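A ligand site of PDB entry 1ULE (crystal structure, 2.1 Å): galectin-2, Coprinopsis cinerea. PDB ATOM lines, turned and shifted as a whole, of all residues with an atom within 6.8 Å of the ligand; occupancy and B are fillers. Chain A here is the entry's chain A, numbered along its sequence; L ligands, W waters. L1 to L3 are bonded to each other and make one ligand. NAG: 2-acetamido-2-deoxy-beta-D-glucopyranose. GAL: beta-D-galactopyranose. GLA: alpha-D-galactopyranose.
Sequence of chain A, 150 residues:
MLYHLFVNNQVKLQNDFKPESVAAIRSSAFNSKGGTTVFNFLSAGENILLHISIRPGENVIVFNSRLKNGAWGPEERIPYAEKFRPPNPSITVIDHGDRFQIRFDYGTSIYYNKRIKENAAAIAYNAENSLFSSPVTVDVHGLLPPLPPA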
ATOM      1  N   THR A  36     -11.192  13.603  28.320  1.00  0.00           N
ATOM      2  CA  THR A  36     -11.561  13.200  26.975  1.00  0.00           C
ATOM      3  C   THR A  36     -12.894  12.462  26.997  1.00  0.00           C
ATOM      4  O   THR A  36     -13.123  11.551  27.789  1.00  0.00           O
ATOM      5  CB  THR A  36     -10.458  12.304  26.361  1.00  0.00           C
ATOM      6  OG1 THR A  36      -9.292  13.099  26.144  1.00  0.00           O
ATOM      7  CG2 THR A  36     -10.914  11.702  25.040  1.00  0.00           C
ATOM      8  N   VAL A  38     -15.789  10.592  24.473  1.00  0.00           N
ATOM      9  CA  VAL A  38     -16.001   9.972  23.175  1.00  0.00           C
ATOM     10  C   VAL A  38     -17.435   9.534  22.875  1.00  0.00           C
ATOM     11  O   VAL A  38     -18.151   9.080  23.757  1.00  0.00           O
ATOM     12  CB  VAL A  38     -15.083   8.718  23.041  1.00  0.00           C
ATOM     13  CG1 VAL A  38     -15.444   7.934  21.794  1.00  0.00           C
ATOM     14  CG2 VAL A  38     -13.625   9.147  23.005  1.00  0.00           C
ATOM     15  N   ASN A  40     -19.362   7.269  19.734  1.00  0.00           N
ATOM     16  CA  ASN A  40     -19.160   6.427  18.553  1.00  0.00           C
ATOM     17  C   ASN A  40     -20.474   6.008  17.938  1.00  0.00           C
ATOM     18  O   ASN A  40     -21.421   5.701  18.648  1.00  0.00           O
ATOM     19  CB  ASN A  40     -18.433   5.110  18.898  1.00  0.00           C
ATOM     20  CG  ASN A  40     -16.982   5.311  19.306  1.00  0.00           C
ATOM     21  OD1 ASN A  40     -16.274   6.130  18.730  1.00  0.00           O
ATOM     22  ND2 ASN A  40     -16.537   4.534  20.283  1.00  0.00           N
ATOM     23  N   HIS A  51     -16.190   8.103  14.863  1.00  0.00           N
ATOM     24  CA  HIS A  51     -15.598   8.235  16.184  1.00  0.00           C
ATOM     25  C   HIS A  51     -15.358   9.726  16.419  1.00  0.00           C
ATOM     26  O   HIS A  51     -14.708  10.398  15.613  1.00  0.00           O
ATOM     27  CB  HIS A  51     -14.274   7.470  16.198  1.00  0.00           C
ATOM     28  CG  HIS A  51     -13.446   7.678  17.435  1.00  0.00           C
ATOM     29  ND1 HIS A  51     -13.788   7.160  18.656  1.00  0.00           N
ATOM     30  CD2 HIS A  51     -12.259   8.306  17.611  1.00  0.00           C
ATOM     31  CE1 HIS A  51     -12.848   7.450  19.538  1.00  0.00           C
ATOM     32  NE2 HIS A  51     -11.900   8.152  18.920  1.00  0.00           N
ATOM     33  N   ILE A  52     -15.919  10.259  17.505  1.00  0.00           N
ATOM     34  CA  ILE A  52     -15.758  11.659  17.855  1.00  0.00           C
ATOM     35  C   ILE A  52     -15.066  11.717  19.219  1.00  0.00           C
ATOM     36  O   ILE A  52     -15.702  11.447  20.240  1.00  0.00           O
ATOM     37  CB  ILE A  52     -17.116  12.388  17.962  1.00  0.00           C
ATOM     38  CG1 ILE A  52     -17.912  12.228  16.667  1.00  0.00           C
ATOM     39  CG2 ILE A  52     -16.891  13.873  18.230  1.00  0.00           C
ATOM     40  CD1 ILE A  52     -19.321  12.792  16.738  1.00  0.00           C
ATOM     41  N   SER A  53     -13.784  12.079  19.210  1.00  0.00           N
ATOM     42  CA  SER A  53     -12.989  12.159  20.435  1.00  0.00           C
ATOM     43  C   SER A  53     -12.768  13.612  20.850  1.00  0.00           C
ATOM     44  O   SER A  53     -11.963  14.325  20.260  1.00  0.00           O
ATOM     45  CB  SER A  53     -11.620  11.485  20.218  1.00  0.00           C
ATOM     46  OG  SER A  53     -10.891  11.422  21.423  1.00  0.00           O
ATOM     47  N   ARG A  55     -11.242  16.154  23.170  1.00  0.00           N
ATOM     48  CA  ARG A  55     -10.122  16.251  24.118  1.00  0.00           C
ATOM     49  C   ARG A  55      -9.840  17.685  24.555  1.00  0.00           C
ATOM     50  O   ARG A  55      -9.127  18.420  23.871  1.00  0.00           O
ATOM     51  CB  ARG A  55      -8.870  15.657  23.475  1.00  0.00           C
ATOM     52  CG  ARG A  55      -9.107  14.318  22.791  1.00  0.00           C
ATOM     53  CD  ARG A  55      -7.880  13.834  22.045  1.00  0.00           C
ATOM     54  NE  ARG A  55      -8.174  12.662  21.214  1.00  0.00           N
ATOM     55  CZ  ARG A  55      -7.299  12.096  20.395  1.00  0.00           C
ATOM     56  NH1 ARG A  55      -6.066  12.568  20.295  1.00  0.00           N
ATOM     57  NH2 ARG A  55      -7.662  11.044  19.666  1.00  0.00           N
ATOM     58  N   GLU A  58      -6.015  18.503  25.178  1.00  0.00           N
ATOM     59  CA  GLU A  58      -5.183  18.618  23.984  1.00  0.00           C
ATOM     60  C   GLU A  58      -5.772  19.711  23.090  1.00  0.00           C
ATOM     61  O   GLU A  58      -5.257  19.973  21.996  1.00  0.00           O
ATOM     62  CB  GLU A  58      -5.177  17.260  23.263  1.00  0.00           C
ATOM     63  CG  GLU A  58      -4.072  17.053  22.235  1.00  0.00           C
ATOM     64  CD  GLU A  58      -4.169  15.688  21.544  1.00  0.00           C
ATOM     65  OE1 GLU A  58      -4.523  14.702  22.226  1.00  0.00           O
ATOM     66  OE2 GLU A  58      -3.876  15.611  20.334  1.00  0.00           O
ATOM     67  N   VAL A  62     -11.174  15.008  17.723  1.00  0.00           N
ATOM     68  CA  VAL A  62     -10.713  14.135  16.657  1.00  0.00           C
ATOM     69  C   VAL A  62     -11.799  13.235  16.074  1.00  0.00           C
ATOM     70  O   VAL A  62     -12.601  12.659  16.805  1.00  0.00           O
ATOM     71  CB  VAL A  62      -9.537  13.271  17.165  1.00  0.00           C
ATOM     72  CG1 VAL A  62      -8.977  12.424  16.027  1.00  0.00           C
ATOM     73  CG2 VAL A  62      -8.460  14.166  17.759  1.00  0.00           C
ATOM     74  N   PHE A  63     -11.798  13.111  14.749  1.00  0.00           N
ATOM     75  CA  PHE A  63     -12.754  12.275  14.039  1.00  0.00           C
ATOM     76  C   PHE A  63     -11.994  11.161  13.320  1.00  0.00           C
ATOM     77  O   PHE A  63     -10.940  11.413  12.737  1.00  0.00           O
ATOM     78  CB  PHE A  63     -13.549  13.090  13.023  1.00  0.00           C
ATOM     79  CG  PHE A  63     -14.301  14.255  13.618  1.00  0.00           C
ATOM     80  CD1 PHE A  63     -13.663  15.474  13.853  1.00  0.00           C
ATOM     81  CD2 PHE A  63     -15.639  14.114  13.987  1.00  0.00           C
ATOM     82  CE1 PHE A  63     -14.352  16.541  14.429  1.00  0.00           C
ATOM     83  CE2 PHE A  63     -16.329  15.180  14.563  1.00  0.00           C
ATOM     84  CZ  PHE A  63     -15.685  16.396  14.791  1.00  0.00           C
ATOM     85  N   ASN A  64     -12.527   9.947  13.349  1.00  0.00           N
ATOM     86  CA  ASN A  64     -11.882   8.802  12.707  1.00  0.00           C
ATOM     87  C   ASN A  64     -12.892   7.657  12.580  1.00  0.00           C
ATOM     88  O   ASN A  64     -14.057   7.793  12.955  1.00  0.00           O
ATOM     89  CB  ASN A  64     -10.683   8.336  13.543  1.00  0.00           C
ATOM     90  CG  ASN A  64      -9.560   7.743  12.697  1.00  0.00           C
ATOM     91  OD1 ASN A  64      -9.803   7.173  11.634  1.00  0.00           O
ATOM     92  ND2 ASN A  64      -8.334   7.856  13.192  1.00  0.00           N
ATOM     93  N   SER A  65     -12.415   6.521  12.060  1.00  0.00           N
ATOM     94  CA  SER A  65     -13.250   5.322  11.901  1.00  0.00           C
ATOM     95  C   SER A  65     -12.328   4.111  12.007  1.00  0.00           C
ATOM     96  O   SER A  65     -11.108   4.241  11.919  1.00  0.00           O
ATOM     97  CB  SER A  65     -13.907   5.289  10.509  1.00  0.00           C
ATOM     98  OG  SER A  65     -14.688   6.441  10.242  1.00  0.00           O
ATOM     99  N   ARG A  66     -12.907   2.928  12.211  1.00  0.00           N
ATOM    100  CA  ARG A  66     -12.121   1.707  12.262  1.00  0.00           C
ATOM    101  C   ARG A  66     -13.026   0.488  12.358  1.00  0.00           C
ATOM    102  O   ARG A  66     -14.095   0.544  12.967  1.00  0.00           O
ATOM    103  CB  ARG A  66     -11.119   1.718  13.433  1.00  0.00           C
ATOM    104  CG  ARG A  66     -11.653   1.233  14.770  1.00  0.00           C
ATOM    105  CD  ARG A  66     -10.511   1.040  15.776  1.00  0.00           C
ATOM    106  NE  ARG A  66     -11.004   0.747  17.126  1.00  0.00           N
ATOM    107  CZ  ARG A  66     -11.426  -0.444  17.532  1.00  0.00           C
ATOM    108  NH1 ARG A  66     -11.419  -1.468  16.706  1.00  0.00           N
ATOM    109  NH2 ARG A  66     -11.881  -0.603  18.765  1.00  0.00           N
ATOM    110  N   TRP A  72      -7.126   2.202  13.496  1.00  0.00           N
ATOM    111  CA  TRP A  72      -7.642   3.534  13.241  1.00  0.00           C
ATOM    112  C   TRP A  72      -7.122   3.990  11.878  1.00  0.00           C
ATOM    113  O   TRP A  72      -6.059   3.573  11.445  1.00  0.00           O
ATOM    114  CB  TRP A  72      -7.153   4.525  14.306  1.00  0.00           C
ATOM    115  CG  TRP A  72      -7.795   4.334  15.655  1.00  0.00           C
ATOM    116  CD1 TRP A  72      -7.190   3.907  16.802  1.00  0.00           C
ATOM    117  CD2 TRP A  72      -9.178   4.513  15.973  1.00  0.00           C
ATOM    118  NE1 TRP A  72      -8.119   3.805  17.815  1.00  0.00           N
ATOM    119  CE2 TRP A  72      -9.348   4.167  17.333  1.00  0.00           C
ATOM    120  CE3 TRP A  72     -10.307   4.924  15.244  1.00  0.00           C
ATOM    121  CZ2 TRP A  72     -10.584   4.224  17.983  1.00  0.00           C
ATOM    122  CZ3 TRP A  72     -11.542   4.986  15.878  1.00  0.00           C
ATOM    123  CH2 TRP A  72     -11.671   4.630  17.237  1.00  0.00           C
ATOM    124  N   GLY A  73      -7.880   4.855  11.201  1.00  0.00           N
ATOM    125  CA  GLY A  73      -7.433   5.359   9.921  1.00  0.00           C
ATOM    126  C   GLY A  73      -6.784   6.705  10.179  1.00  0.00           C
ATOM    127  O   GLY A  73      -6.406   6.993  11.307  1.00  0.00           O
ATOM    128  N   PRO A  74      -6.614   7.555   9.152  1.00  0.00           N
ATOM    129  CA  PRO A  74      -6.003   8.876   9.348  1.00  0.00           C
ATOM    130  C   PRO A  74      -6.974   9.790  10.098  1.00  0.00           C
ATOM    131  O   PRO A  74      -8.187   9.694   9.896  1.00  0.00           O
ATOM    132  CB  PRO A  74      -5.722   9.347   7.925  1.00  0.00           C
ATOM    133  CG  PRO A  74      -6.815   8.677   7.129  1.00  0.00           C
ATOM    134  CD  PRO A  74      -6.828   7.290   7.719  1.00  0.00           C
ATOM    135  N   GLU A  75      -6.458  10.655  10.955  1.00  0.00           N
ATOM    136  CA  GLU A  75      -7.303  11.543  11.745  1.00  0.00           C
ATOM    137  C   GLU A  75      -7.691  12.829  11.033  1.00  0.00           C
ATOM    138  O   GLU A  75      -6.987  13.322  10.161  1.00  0.00           O
ATOM    139  CB  GLU A  75      -6.615  11.910  13.057  1.00  0.00           C
ATOM    140  CG  GLU A  75      -6.207  10.736  13.939  1.00  0.00           C
ATOM    141  CD  GLU A  75      -5.639  11.176  15.279  1.00  0.00           C
ATOM    142  OE1 GLU A  75      -4.957  12.216  15.322  1.00  0.00           O
ATOM    143  OE2 GLU A  75      -5.868  10.465  16.289  1.00  0.00           O
ATOM    144  N   GLU A  76      -8.853  13.351  11.420  1.00  0.00           N
ATOM    145  CA  GLU A  76      -9.367  14.609  10.905  1.00  0.00           C
ATOM    146  C   GLU A  76      -9.610  15.398  12.184  1.00  0.00           C
ATOM    147  O   GLU A  76     -10.353  14.951  13.067  1.00  0.00           O
ATOM    148  CB  GLU A  76     -10.632  14.384  10.077  1.00  0.00           C
ATOM    149  CG  GLU A  76     -10.308  13.696   8.740  1.00  0.00           C
ATOM    150  CD  GLU A  76     -11.528  13.362   7.883  1.00  0.00           C
ATOM    151  OE1 GLU A  76     -12.398  14.242   7.710  1.00  0.00           O
ATOM    152  OE2 GLU A  76     -11.607  12.221   7.369  1.00  0.00           O
ATOM    153  N   ARG A  77      -8.970  16.551  12.298  1.00  0.00           N
ATOM    154  CA  ARG A  77      -9.048  17.361  13.505  1.00  0.00           C
ATOM    155  C   ARG A  77      -9.581  18.785  13.372  1.00  0.00           C
ATOM    156  O   ARG A  77      -9.598  19.366  12.292  1.00  0.00           O
ATOM    157  CB  ARG A  77      -7.671  17.448  14.149  1.00  0.00           C
ATOM    158  CG  ARG A  77      -7.043  16.115  14.504  1.00  0.00           C
ATOM    159  CD  ARG A  77      -5.585  16.290  14.905  1.00  0.00           C
ATOM    160  NE  ARG A  77      -5.046  15.087  15.527  1.00  0.00           N
ATOM    161  CZ  ARG A  77      -4.598  15.034  16.784  1.00  0.00           C
ATOM    162  NH1 ARG A  77      -4.613  16.121  17.537  1.00  0.00           N
ATOM    163  NH2 ARG A  77      -4.150  13.892  17.275  1.00  0.00           N
ATOM    164  N   ASN A 126     -18.382   7.092  25.783  1.00  0.00           N
ATOM    165  CA  ASN A 126     -17.350   6.650  26.721  1.00  0.00           C
ATOM    166  C   ASN A 126     -16.550   7.797  27.344  1.00  0.00           C
ATOM    167  O   ASN A 126     -16.234   8.776  26.677  1.00  0.00           O
ATOM    168  CB  ASN A 126     -16.364   5.700  26.034  1.00  0.00           C
ATOM    169  CG  ASN A 126     -17.055   4.520  25.394  1.00  0.00           C
ATOM    170  OD1 ASN A 126     -17.777   3.780  26.058  1.00  0.00           O
ATOM    171  ND2 ASN A 126     -16.834   4.340  24.092  1.00  0.00           N
HETATM  172  C1  NAG L   1      -1.109   9.460  18.432  1.00  0.00           C
HETATM  173  C2  NAG L   1      -2.229  10.395  17.976  1.00  0.00           C
HETATM  174  C3  NAG L   1      -3.423  10.207  18.907  1.00  0.00           C
HETATM  175  C4  NAG L   1      -3.846   8.741  18.918  1.00  0.00           C
HETATM  176  C5  NAG L   1      -2.640   7.844  19.268  1.00  0.00           C
HETATM  177  C6  NAG L   1      -2.941   6.352  19.199  1.00  0.00           C
HETATM  178  C7  NAG L   1      -1.409  12.378  16.866  1.00  0.00           C
HETATM  179  C8  NAG L   1      -1.079  13.868  16.948  1.00  0.00           C
HETATM  180  N2  NAG L   1      -1.775  11.778  17.997  1.00  0.00           N
HETATM  181  O1  NAG L   1      -0.028   9.595  17.578  1.00  0.00           O
HETATM  182  O3  NAG L   1      -4.515  11.018  18.490  1.00  0.00           O
HETATM  183  O4  NAG L   1      -4.876   8.564  19.901  1.00  0.00           O
HETATM  184  O5  NAG L   1      -1.559   8.100  18.358  1.00  0.00           O
HETATM  185  O6  NAG L   1      -3.510   5.988  17.946  1.00  0.00           O
HETATM  186  O7  NAG L   1      -1.349  11.795  15.788  1.00  0.00           O
HETATM  187  C1  GAL L   2      -5.938   7.758  19.531  1.00  0.00           C
HETATM  188  C2  GAL L   2      -6.774   7.481  20.758  1.00  0.00           C
HETATM  189  C3  GAL L   2      -7.983   6.647  20.362  1.00  0.00           C
HETATM  190  C4  GAL L   2      -8.783   7.342  19.252  1.00  0.00           C
HETATM  191  C5  GAL L   2      -7.838   7.666  18.079  1.00  0.00           C
HETATM  192  C6  GAL L   2      -8.517   8.459  16.989  1.00  0.00           C
HETATM  193  O2  GAL L   2      -5.983   6.774  21.708  1.00  0.00           O
HETATM  194  O3  GAL L   2      -8.825   6.442  21.512  1.00  0.00           O
HETATM  195  O4  GAL L   2      -9.369   8.537  19.742  1.00  0.00           O
HETATM  196  O5  GAL L   2      -6.713   8.449  18.547  1.00  0.00           O
HETATM  197  O6  GAL L   2      -7.634   8.648  15.884  1.00  0.00           O
HETATM  198  C1  GLA L   3      -9.666   5.323  21.447  1.00  0.00           C
HETATM  199  C2  GLA L   3     -10.378   5.144  22.784  1.00  0.00           C
HETATM  200  C3  GLA L   3      -9.375   4.712  23.850  1.00  0.00           C
HETATM  201  C4  GLA L   3      -8.644   3.450  23.395  1.00  0.00           C
HETATM  202  C5  GLA L   3      -7.981   3.697  22.033  1.00  0.00           C
HETATM  203  C6  GLA L   3      -7.314   2.455  21.466  1.00  0.00           C
HETATM  204  O2  GLA L   3     -10.972   6.380  23.172  1.00  0.00           O
HETATM  205  O3  GLA L   3     -10.059   4.460  25.066  1.00  0.00           O
HETATM  206  O4  GLA L   3      -9.569   2.379  23.286  1.00  0.00           O
HETATM  207  O5  GLA L   3      -8.972   4.134  21.077  1.00  0.00           O
HETATM  208  O6  GLA L   3      -6.616   2.761  20.260  1.00  0.00           O
HETATM  209  O   HOH W   1     -12.442   6.739  25.595  1.00  0.00           O
HETATM  210  O   HOH W   2      -8.296  -0.014  24.636  1.00  0.00           O
HETATM  211  O   HOH W   3      -4.656   4.229  21.782  1.00  0.00           O
HETATM  212  O   HOH W   4      -2.815  12.564  13.754  1.00  0.00           O
HETATM  213  O   HOH W   5     -10.955   0.850  21.680  1.00  0.00           O
HETATM  214  O   HOH W   6     -13.681   5.231  23.845  1.00  0.00           O
HETATM  215  O   HOH W   7      -0.066   7.415  15.593  1.00  0.00           O
HETATM  216  O   HOH W   8      -5.066   7.084  15.700  1.00  0.00           O
HETATM  217  O   HOH W   9      -9.962   9.160  22.394  1.00  0.00           O
HETATM  218  O   HOH W  10      -2.449  13.305  20.023  1.00  0.00           O
HETATM  219  O   HOH W  11     -12.572   2.524  24.855  1.00  0.00           O
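An oxygen (O6) of GAL L2 lies within hydrogen-bond range of the side-chain carboxylate (OE2) of Glu 75 (2.6 Å).
An oxygen (O4) of GAL L2 sits at hydrogen-bond distance from a ring nitrogen (NE2) of His 51 (2.7 Å).
The guanidinium group of Arg 55 lies within hydrogen-bond range of an oxygen (O3) of NAG L1 (2.8 Å).
The side-chain amide nitrogen of Asn 64 sits at hydrogen-bond distance from an oxygen (O6) of GAL L2, 2.9 Å away.
The indole nitrogen of Trp 72 is in hydrogen-bond range of an oxygen (O6) of GLA L3, at 3.1 Å.
The guanidinium group (NH2) of Arg 77 sits close to an oxygen (O3) of NAG L1 (3.1 Å).
OE1 of Glu 75 lies within salt-bridge range of NH2 of Arg 77, at 2.7 Å.
The backbone NH of His 51 sits at hydrogen-bond distance from the backbone carbonyl oxygen of Asn 64 (2.9 Å).
The side-chain amide oxygen (OD1) of Asn 40 lies within hydrogen-bond range of a ring nitrogen (ND1) of His 51 (2.7 Å).
The guanidinium group of Arg 55 is in hydrogen-bond range of the side-chain hydroxyl of Ser 53, 3.0 Å away.
The guanidinium group (NH1) of Arg 55 is in salt-bridge range of the side-chain carboxylate (OE1) of Glu 58 (3.3 Å).
O of Gly 73 is in hydrogen-bond range of ND2 of Asn 64.
The guanidinium group of Arg 77 is in salt-bridge range of the side-chain carboxylate of Glu 58.
O of Val 38 sits at hydrogen-bond distance from N of Asn 126 (2.8 Å).
Merely in contact with the ligand: Val 38 (3.8 Å) and Ser 53 (3.7 Å).
Hydrophobic or aromatic side chains that line the ligand: Val 38, His 51 and Trp 72.
Of the 20 residues printed, 8 come within 4 Å of the ligand.
The nearest printed residue that does not touch the ligand is Val 62 (4.01 Å).
Water W5 lies within hydrogen-bond range of O4 of GLA L3 (2.6 Å) and NH2 of Arg 66 (3.4 Å).
Water W4 lies within hydrogen-bond range of O7 of NAG L1 (2.6 Å) and OE1 of Glu 75 (2.7 Å).
Water W10 lies within hydrogen-bond range of a nitrogen (N2) of NAG L1 (2.6 Å), the side-chain carboxylate of Glu 58 (2.7 Å) and the guanidinium group of Arg 77 (3.3 Å).
Water W9 bridges OG of Ser 53 (2.6 Å) and O4 of GAL L2 (2.8 Å).
Water W6 bridges an oxygen (O2) of GLA L3 (3.0 Å) and the side-chain amide nitrogen of Asn 126 (3.3 Å).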
